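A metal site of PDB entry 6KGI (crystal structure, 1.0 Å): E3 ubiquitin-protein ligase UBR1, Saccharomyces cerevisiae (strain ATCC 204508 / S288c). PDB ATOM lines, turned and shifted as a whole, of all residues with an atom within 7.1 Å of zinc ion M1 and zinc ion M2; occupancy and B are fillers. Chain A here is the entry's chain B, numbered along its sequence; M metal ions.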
ATOM      1  N   HIS A   8       5.354  18.040  28.047  1.00  0.00           N
ATOM      2  CA  HIS A   8       6.801  18.127  27.947  1.00  0.00           C
ATOM      3  C   HIS A   8       7.323  19.510  28.295  1.00  0.00           C
ATOM      4  O   HIS A   8       8.539  19.717  28.308  1.00  0.00           O
ATOM      5  CB  HIS A   8       7.267  17.738  26.544  1.00  0.00           C
ATOM      6  CG  HIS A   8       6.791  16.383  26.127  1.00  0.00           C
ATOM      7  ND1 HIS A   8       5.693  16.206  25.318  1.00  0.00           N
ATOM      8  CD2 HIS A   8       7.252  15.154  26.429  1.00  0.00           C
ATOM      9  CE1 HIS A   8       5.510  14.907  25.131  1.00  0.00           C
ATOM     10  NE2 HIS A   8       6.443  14.251  25.785  1.00  0.00           N
ATOM     11  N   LYS A   9       6.442  20.467  28.564  1.00  0.00           N
ATOM     12  CA  LYS A   9       6.865  21.789  28.979  1.00  0.00           C
ATOM     13  C   LYS A   9       7.708  21.680  30.237  1.00  0.00           C
ATOM     14  O   LYS A   9       7.375  20.937  31.160  1.00  0.00           O
ATOM     15  CB  LYS A   9       5.631  22.655  29.243  1.00  0.00           C
ATOM     16  CG  LYS A   9       5.904  24.047  29.780  1.00  0.00           C
ATOM     17  CD  LYS A   9       4.621  24.839  29.943  1.00  0.00           C
ATOM     18  CE  LYS A   9       4.846  26.175  30.599  1.00  0.00           C
ATOM     19  NZ  LYS A   9       3.596  26.967  30.642  1.00  0.00           N
ATOM     20  N   HIS A  10       8.802  22.445  30.287  1.00  0.00           N
ATOM     21  CA  HIS A  10       9.717  22.356  31.413  1.00  0.00           C
ATOM     22  C   HIS A  10      10.313  23.723  31.756  1.00  0.00           C
ATOM     23  O   HIS A  10      11.431  23.810  32.267  1.00  0.00           O
ATOM     24  CB  HIS A  10      10.811  21.334  31.150  1.00  0.00           C
ATOM     25  CG  HIS A  10      11.647  21.675  29.956  1.00  0.00           C
ATOM     26  ND1 HIS A  10      12.762  22.474  30.043  1.00  0.00           N
ATOM     27  CD2 HIS A  10      11.508  21.363  28.640  1.00  0.00           C
ATOM     28  CE1 HIS A  10      13.291  22.627  28.831  1.00  0.00           C
ATOM     29  NE2 HIS A  10      12.542  21.966  27.965  1.00  0.00           N
ATOM     30  N   THR A  11       9.558  24.789  31.485  1.00  0.00           N
ATOM     31  CA  THR A  11       9.937  26.126  31.899  1.00  0.00           C
ATOM     32  C   THR A  11      10.447  26.093  33.323  1.00  0.00           C
ATOM     33  O   THR A  11       9.815  25.485  34.196  1.00  0.00           O
ATOM     34  CB  THR A  11       8.707  27.028  31.824  1.00  0.00           C
ATOM     35  OG1 THR A  11       8.038  26.819  30.576  1.00  0.00           O
ATOM     36  CG2 THR A  11       9.075  28.511  31.983  1.00  0.00           C
ATOM     37  N   ARG A  13      13.468  24.813  34.261  1.00  0.00           N
ATOM     38  CA  ARG A  13      14.449  23.768  34.490  1.00  0.00           C
ATOM     39  C   ARG A  13      14.972  23.267  33.151  1.00  0.00           C
ATOM     40  O   ARG A  13      14.442  23.596  32.082  1.00  0.00           O
ATOM     41  CB  ARG A  13      13.858  22.598  35.280  1.00  0.00           C
ATOM     42  CG  ARG A  13      12.726  21.898  34.536  1.00  0.00           C
ATOM     43  CD  ARG A  13      12.157  20.762  35.350  1.00  0.00           C
ATOM     44  NE  ARG A  13      11.010  20.111  34.747  1.00  0.00           N
ATOM     45  CZ  ARG A  13      11.071  19.149  33.835  1.00  0.00           C
ATOM     46  NH1 ARG A  13      12.245  18.737  33.354  1.00  0.00           N
ATOM     47  NH2 ARG A  13       9.950  18.591  33.404  1.00  0.00           N
ATOM     48  N   ASN A  14      16.013  22.434  33.221  1.00  0.00           N
ATOM     49  CA  ASN A  14      16.453  21.687  32.061  1.00  0.00           C
ATOM     50  C   ASN A  14      15.461  20.572  31.743  1.00  0.00           C
ATOM     51  O   ASN A  14      14.813  20.020  32.636  1.00  0.00           O
ATOM     52  CB  ASN A  14      17.815  21.051  32.327  1.00  0.00           C
ATOM     53  CG  ASN A  14      17.761  20.032  33.470  1.00  0.00           C
ATOM     54  OD1 ASN A  14      17.378  20.367  34.599  1.00  0.00           O
ATOM     55  ND2 ASN A  14      18.117  18.790  33.166  1.00  0.00           N
ATOM     56  N   CYS A  15      15.367  20.215  30.463  1.00  0.00           N
ATOM     57  CA  CYS A  15      14.466  19.141  30.056  1.00  0.00           C
ATOM     58  C   CYS A  15      14.861  17.811  30.694  1.00  0.00           C
ATOM     59  O   CYS A  15      14.080  17.198  31.441  1.00  0.00           O
ATOM     60  CB  CYS A  15      14.478  19.012  28.527  1.00  0.00           C
ATOM     61  SG  CYS A  15      13.516  17.573  27.966  1.00  0.00           S
ATOM     62  N   GLY A  16      16.081  17.360  30.419  1.00  0.00           N
ATOM     63  CA  GLY A  16      16.613  16.162  31.027  1.00  0.00           C
ATOM     64  C   GLY A  16      16.025  14.861  30.558  1.00  0.00           C
ATOM     65  O   GLY A  16      16.323  13.818  31.153  1.00  0.00           O
ATOM     66  N   ARG A  17      15.205  14.857  29.512  1.00  0.00           N
ATOM     67  CA  ARG A  17      14.622  13.622  29.015  1.00  0.00           C
ATOM     68  C   ARG A  17      15.732  12.644  28.633  1.00  0.00           C
ATOM     69  O   ARG A  17      16.661  13.003  27.902  1.00  0.00           O
ATOM     70  CB  ARG A  17      13.756  13.903  27.793  1.00  0.00           C
ATOM     71  CG  ARG A  17      13.103  12.684  27.188  1.00  0.00           C
ATOM     72  CD  ARG A  17      12.397  13.038  25.894  1.00  0.00           C
ATOM     73  NE  ARG A  17      11.562  11.930  25.446  1.00  0.00           N
ATOM     74  CZ  ARG A  17      10.396  11.625  25.985  1.00  0.00           C
ATOM     75  NH1 ARG A  17       9.902  12.362  26.980  1.00  0.00           N
ATOM     76  NH2 ARG A  17       9.702  10.592  25.521  1.00  0.00           N
ATOM     77  N   PHE A  19      16.923   9.528  26.501  1.00  0.00           N
ATOM     78  CA  PHE A  19      16.518   8.929  25.237  1.00  0.00           C
ATOM     79  C   PHE A  19      16.399   7.418  25.361  1.00  0.00           C
ATOM     80  O   PHE A  19      17.174   6.773  26.075  1.00  0.00           O
ATOM     81  CB  PHE A  19      17.534   9.288  24.156  1.00  0.00           C
ATOM     82  CG  PHE A  19      17.660  10.754  23.939  1.00  0.00           C
ATOM     83  CD1 PHE A  19      16.665  11.456  23.290  1.00  0.00           C
ATOM     84  CD2 PHE A  19      18.758  11.443  24.420  1.00  0.00           C
ATOM     85  CE1 PHE A  19      16.768  12.818  23.114  1.00  0.00           C
ATOM     86  CE2 PHE A  19      18.867  12.799  24.238  1.00  0.00           C
ATOM     87  CZ  PHE A  19      17.869  13.489  23.595  1.00  0.00           C
ATOM     88  N   VAL A  38      22.377  18.232  22.555  1.00  0.00           N
ATOM     89  CA  VAL A  38      21.266  17.635  21.827  1.00  0.00           C
ATOM     90  C   VAL A  38      19.921  18.126  22.338  1.00  0.00           C
ATOM     91  O   VAL A  38      19.784  18.584  23.484  1.00  0.00           O
ATOM     92  CB  VAL A  38      21.302  16.089  21.878  1.00  0.00           C
ATOM     93  CG1 VAL A  38      22.557  15.553  21.214  1.00  0.00           C
ATOM     94  CG2 VAL A  38      21.213  15.604  23.328  1.00  0.00           C
ATOM     95  N   LEU A  39      18.923  17.981  21.469  1.00  0.00           N
ATOM     96  CA  LEU A  39      17.550  18.354  21.767  1.00  0.00           C
ATOM     97  C   LEU A  39      16.609  17.219  21.414  1.00  0.00           C
ATOM     98  O   LEU A  39      16.665  16.656  20.307  1.00  0.00           O
ATOM     99  CB  LEU A  39      17.141  19.594  20.965  1.00  0.00           C
ATOM    100  CG  LEU A  39      17.905  20.871  21.312  1.00  0.00           C
ATOM    101  CD1 LEU A  39      17.735  21.934  20.241  1.00  0.00           C
ATOM    102  CD2 LEU A  39      17.468  21.400  22.668  1.00  0.00           C
ATOM    103  N   CYS A  40      15.703  16.900  22.337  1.00  0.00           N
ATOM    104  CA  CYS A  40      14.689  15.886  22.075  1.00  0.00           C
ATOM    105  C   CYS A  40      13.639  16.431  21.118  1.00  0.00           C
ATOM    106  O   CYS A  40      13.563  17.623  20.836  1.00  0.00           O
ATOM    107  CB  CYS A  40      14.057  15.413  23.387  1.00  0.00           C
ATOM    108  SG  CYS A  40      12.817  16.529  24.106  1.00  0.00           S
ATOM    109  N   ILE A  41      12.829  15.510  20.588  1.00  0.00           N
ATOM    110  CA  ILE A  41      11.848  15.881  19.575  1.00  0.00           C
ATOM    111  C   ILE A  41      10.785  16.820  20.136  1.00  0.00           C
ATOM    112  O   ILE A  41      10.159  17.559  19.386  1.00  0.00           O
ATOM    113  CB  ILE A  41      11.202  14.628  18.942  1.00  0.00           C
ATOM    114  CG1 ILE A  41      10.434  13.811  19.984  1.00  0.00           C
ATOM    115  CG2 ILE A  41      12.236  13.807  18.219  1.00  0.00           C
ATOM    116  CD1 ILE A  41       9.733  12.594  19.427  1.00  0.00           C
ATOM    117  N   HIS A  42      10.518  16.759  21.442  1.00  0.00           N
ATOM    118  CA  HIS A  42       9.497  17.600  22.046  1.00  0.00           C
ATOM    119  C   HIS A  42       9.978  19.028  22.244  1.00  0.00           C
ATOM    120  O   HIS A  42       9.159  19.945  22.373  1.00  0.00           O
ATOM    121  CB  HIS A  42       9.054  16.988  23.370  1.00  0.00           C
ATOM    122  CG  HIS A  42       8.737  15.538  23.241  1.00  0.00           C
ATOM    123  ND1 HIS A  42       7.636  15.097  22.542  1.00  0.00           N
ATOM    124  CD2 HIS A  42       9.407  14.438  23.642  1.00  0.00           C
ATOM    125  CE1 HIS A  42       7.631  13.772  22.552  1.00  0.00           C
ATOM    126  NE2 HIS A  42       8.697  13.349  23.206  1.00  0.00           N
ATOM    127  N   CYS A  43      11.285  19.218  22.268  1.00  0.00           N
ATOM    128  CA  CYS A  43      11.912  20.503  22.547  1.00  0.00           C
ATOM    129  C   CYS A  43      12.413  21.209  21.303  1.00  0.00           C
ATOM    130  O   CYS A  43      12.325  22.445  21.227  1.00  0.00           O
ATOM    131  CB  CYS A  43      13.101  20.297  23.490  1.00  0.00           C
ATOM    132  SG  CYS A  43      12.583  19.881  25.153  1.00  0.00           S
ATOM    133  N   PHE A  44      12.976  20.474  20.346  1.00  0.00           N
ATOM    134  CA  PHE A  44      13.568  21.104  19.183  1.00  0.00           C
ATOM    135  C   PHE A  44      12.543  21.988  18.485  1.00  0.00           C
ATOM    136  O   PHE A  44      11.463  21.526  18.119  1.00  0.00           O
ATOM    137  CB  PHE A  44      14.055  20.042  18.192  1.00  0.00           C
ATOM    138  CG  PHE A  44      14.621  20.631  16.921  1.00  0.00           C
ATOM    139  CD1 PHE A  44      15.937  21.064  16.869  1.00  0.00           C
ATOM    140  CD2 PHE A  44      13.836  20.764  15.793  1.00  0.00           C
ATOM    141  CE1 PHE A  44      16.462  21.633  15.710  1.00  0.00           C
ATOM    142  CE2 PHE A  44      14.353  21.326  14.633  1.00  0.00           C
ATOM    143  CZ  PHE A  44      15.669  21.758  14.595  1.00  0.00           C
ATOM    144  N   ILE A  66      20.915  12.654  27.672  1.00  0.00           N
ATOM    145  CA  ILE A  66      19.707  13.395  27.985  1.00  0.00           C
ATOM    146  C   ILE A  66      19.606  14.648  27.137  1.00  0.00           C
ATOM    147  O   ILE A  66      20.601  15.183  26.651  1.00  0.00           O
ATOM    148  CB  ILE A  66      19.623  13.775  29.486  1.00  0.00           C
ATOM    149  CG1 ILE A  66      20.739  14.755  29.864  1.00  0.00           C
ATOM    150  CG2 ILE A  66      19.689  12.527  30.361  1.00  0.00           C
ATOM    151  CD1 ILE A  66      20.694  15.196  31.324  1.00  0.00           C
ATOM    152  N   CYS A  67      18.375  15.138  27.001  1.00  0.00           N
ATOM    153  CA  CYS A  67      18.111  16.388  26.289  1.00  0.00           C
ATOM    154  C   CYS A  67      18.656  17.580  27.075  1.00  0.00           C
ATOM    155  O   CYS A  67      18.414  17.707  28.285  1.00  0.00           O
ATOM    156  CB  CYS A  67      16.606  16.561  26.121  1.00  0.00           C
ATOM    157  SG  CYS A  67      16.120  18.109  25.347  1.00  0.00           S
ATOM    158  N   ASP A  68      19.331  18.472  26.355  1.00  0.00           N
ATOM    159  CA  ASP A  68      19.961  19.646  26.945  1.00  0.00           C
ATOM    160  C   ASP A  68      19.122  20.924  26.822  1.00  0.00           C
ATOM    161  O   ASP A  68      19.624  22.009  27.145  1.00  0.00           O
ATOM    162  CB  ASP A  68      21.321  19.894  26.292  1.00  0.00           C
ATOM    163  CG  ASP A  68      22.276  18.738  26.462  1.00  0.00           C
ATOM    164  OD1 ASP A  68      22.611  18.412  27.637  1.00  0.00           O
ATOM    165  OD2 ASP A  68      22.700  18.152  25.437  1.00  0.00           O
ATOM    166  N   CYS A  69      17.873  20.835  26.370  1.00  0.00           N
ATOM    167  CA  CYS A  69      17.037  22.026  26.296  1.00  0.00           C
ATOM    168  C   CYS A  69      16.917  22.652  27.684  1.00  0.00           C
ATOM    169  O   CYS A  69      16.677  21.956  28.661  1.00  0.00           O
ATOM    170  CB  CYS A  69      15.653  21.640  25.759  1.00  0.00           C
ATOM    171  SG  CYS A  69      14.622  23.100  25.362  1.00  0.00           S
ATOM    172  N   GLY A  70      17.121  23.962  27.780  1.00  0.00           N
ATOM    173  CA  GLY A  70      17.039  24.625  29.057  1.00  0.00           C
ATOM    174  C   GLY A  70      18.336  24.640  29.843  1.00  0.00           C
ATOM    175  O   GLY A  70      18.364  25.219  30.946  1.00  0.00           O
ATOM    176  N   HIS A  80      13.958  28.501  22.190  1.00  0.00           N
ATOM    177  CA  HIS A  80      12.548  28.714  22.541  1.00  0.00           C
ATOM    178  C   HIS A  80      11.887  27.357  22.444  1.00  0.00           C
ATOM    179  O   HIS A  80      11.483  26.928  21.365  1.00  0.00           O
ATOM    180  CB  HIS A  80      11.951  29.765  21.625  1.00  0.00           C
ATOM    181  CG  HIS A  80      12.729  31.027  21.634  1.00  0.00           C
ATOM    182  ND1 HIS A  80      13.854  31.201  20.866  1.00  0.00           N
ATOM    183  CD2 HIS A  80      12.590  32.169  22.361  1.00  0.00           C
ATOM    184  CE1 HIS A  80      14.365  32.405  21.084  1.00  0.00           C
ATOM    185  NE2 HIS A  80      13.621  33.012  21.992  1.00  0.00           N
ATOM    186  N   CYS A  81      11.808  26.680  23.588  1.00  0.00           N
ATOM    187  CA  CYS A  81      11.366  25.288  23.611  1.00  0.00           C
ATOM    188  C   CYS A  81      10.038  25.120  22.894  1.00  0.00           C
ATOM    189  O   CYS A  81       9.073  25.838  23.165  1.00  0.00           O
ATOM    190  CB  CYS A  81      11.244  24.820  25.053  1.00  0.00           C
ATOM    191  SG  CYS A  81      10.703  23.103  25.197  1.00  0.00           S
ATOM    192  N   LYS A  82       9.978  24.134  21.992  1.00  0.00           N
ATOM    193  CA  LYS A  82       8.735  23.912  21.262  1.00  0.00           C
ATOM    194  C   LYS A  82       7.586  23.575  22.212  1.00  0.00           C
ATOM    195  O   LYS A  82       6.436  23.952  21.958  1.00  0.00           O
ATOM    196  CB  LYS A  82       8.927  22.787  20.247  1.00  0.00           C
ATOM    197  CG  LYS A  82       7.743  22.642  19.308  1.00  0.00           C
ATOM    198  CD  LYS A  82       7.974  21.577  18.266  1.00  0.00           C
ATOM    199  CE  LYS A  82       7.918  20.206  18.903  1.00  0.00           C
ATOM    200  NZ  LYS A  82       7.845  19.142  17.873  1.00  0.00           N
ATOM    201  N   ALA A  83       7.881  22.888  23.319  1.00  0.00           N
ATOM    202  CA  ALA A  83       6.840  22.490  24.251  1.00  0.00           C
ATOM    203  C   ALA A  83       6.258  23.651  25.041  1.00  0.00           C
ATOM    204  O   ALA A  83       5.217  23.471  25.691  1.00  0.00           O
ATOM    205  CB  ALA A  83       7.381  21.434  25.214  1.00  0.00           C
ATOM    206  N   GLU A  84       6.899  24.811  25.016  1.00  0.00           N
ATOM    207  CA  GLU A  84       6.343  25.995  25.652  1.00  0.00           C
ATOM    208  C   GLU A  84       5.364  26.719  24.741  1.00  0.00           C
ATOM    209  O   GLU A  84       4.556  27.513  25.238  1.00  0.00           O
ATOM    210  CB  GLU A  84       7.480  26.956  26.002  1.00  0.00           C
ATOM    211  CG  GLU A  84       7.359  27.641  27.334  1.00  0.00           C
ATOM    212  CD  GLU A  84       8.590  28.456  27.686  1.00  0.00           C
ATOM    213  OE1 GLU A  84       8.678  29.610  27.225  1.00  0.00           O
ATOM    214  OE2 GLU A  84       9.460  27.941  28.425  1.00  0.00           O
HETATM  215 ZN    ZN M   1      13.828  17.922  25.673  1.00  0.00          ZN
HETATM  216 ZN    ZN M   2      12.625  22.093  25.938  1.00  0.00          ZN
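A ring nitrogen (ND1) of His 10 sits at hydrogen-bond distance from the backbone NH (N) of Cys 15 (3.5 Å).
A ring nitrogen (ND1) of His 10 is in hydrogen-bond range of the backbone carbonyl oxygen of Arg 13, at 2.9 Å.
The side-chain sulfur (SG) of Cys 81 lies close to the backbone NH (N) of Ala 83, 3.4 Å away.
The side-chain sulfur (SG) of Cys 67 lies close to the backbone NH (N) of Cys 69, at 3.4 Å.
O of Cys 69 sits at hydrogen-bond distance from N of Cys 15.
The backbone carbonyl oxygen (O) of Cys 67 lies within hydrogen-bond range of the backbone NH (N) of Gly 16, at 3.2 Å.
The backbone NH (N) of His 42 sits close to the side-chain sulfur (SG) of Cys 40 (3.5 Å).
O of Cys 15 is in hydrogen-bond range of NH1 of Arg 13, 3.1 Å away.
Of the 27 residues printed, 4 come within 4 Å of zinc ion M1.
The nearest printed residue that does not touch zinc ion M1 is Cys 69 (4.1 Å).
Four residues have an atom within 4 Å of zinc ion M2: His 10, Cys 43, Cys 69 and Cys 81.
Along chain A the residues within 4 Å of zinc ion M2 span positions 10 to 81.
Zinc ion M1 is bound by the side-chain sulfur (SG) of Cys 67 (2.3 Å), the side-chain sulfur (SG) of Cys 40 (2.3 Å), the side-chain sulfur (SG) of Cys 15 (2.3 Å) and the side-chain sulfur (SG) of Cys 43 (2.4 Å).
Zinc ion M1 has four donor atoms within binding distance.
Zinc ion M2 is bound by a ring nitrogen (NE2) of His 10 (2.0 Å), the side-chain sulfur (SG) of Cys 81 (2.3 Å), the side-chain sulfur (SG) of Cys 69 (2.3 Å) and the side-chain sulfur (SG) of Cys 43 (2.3 Å).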
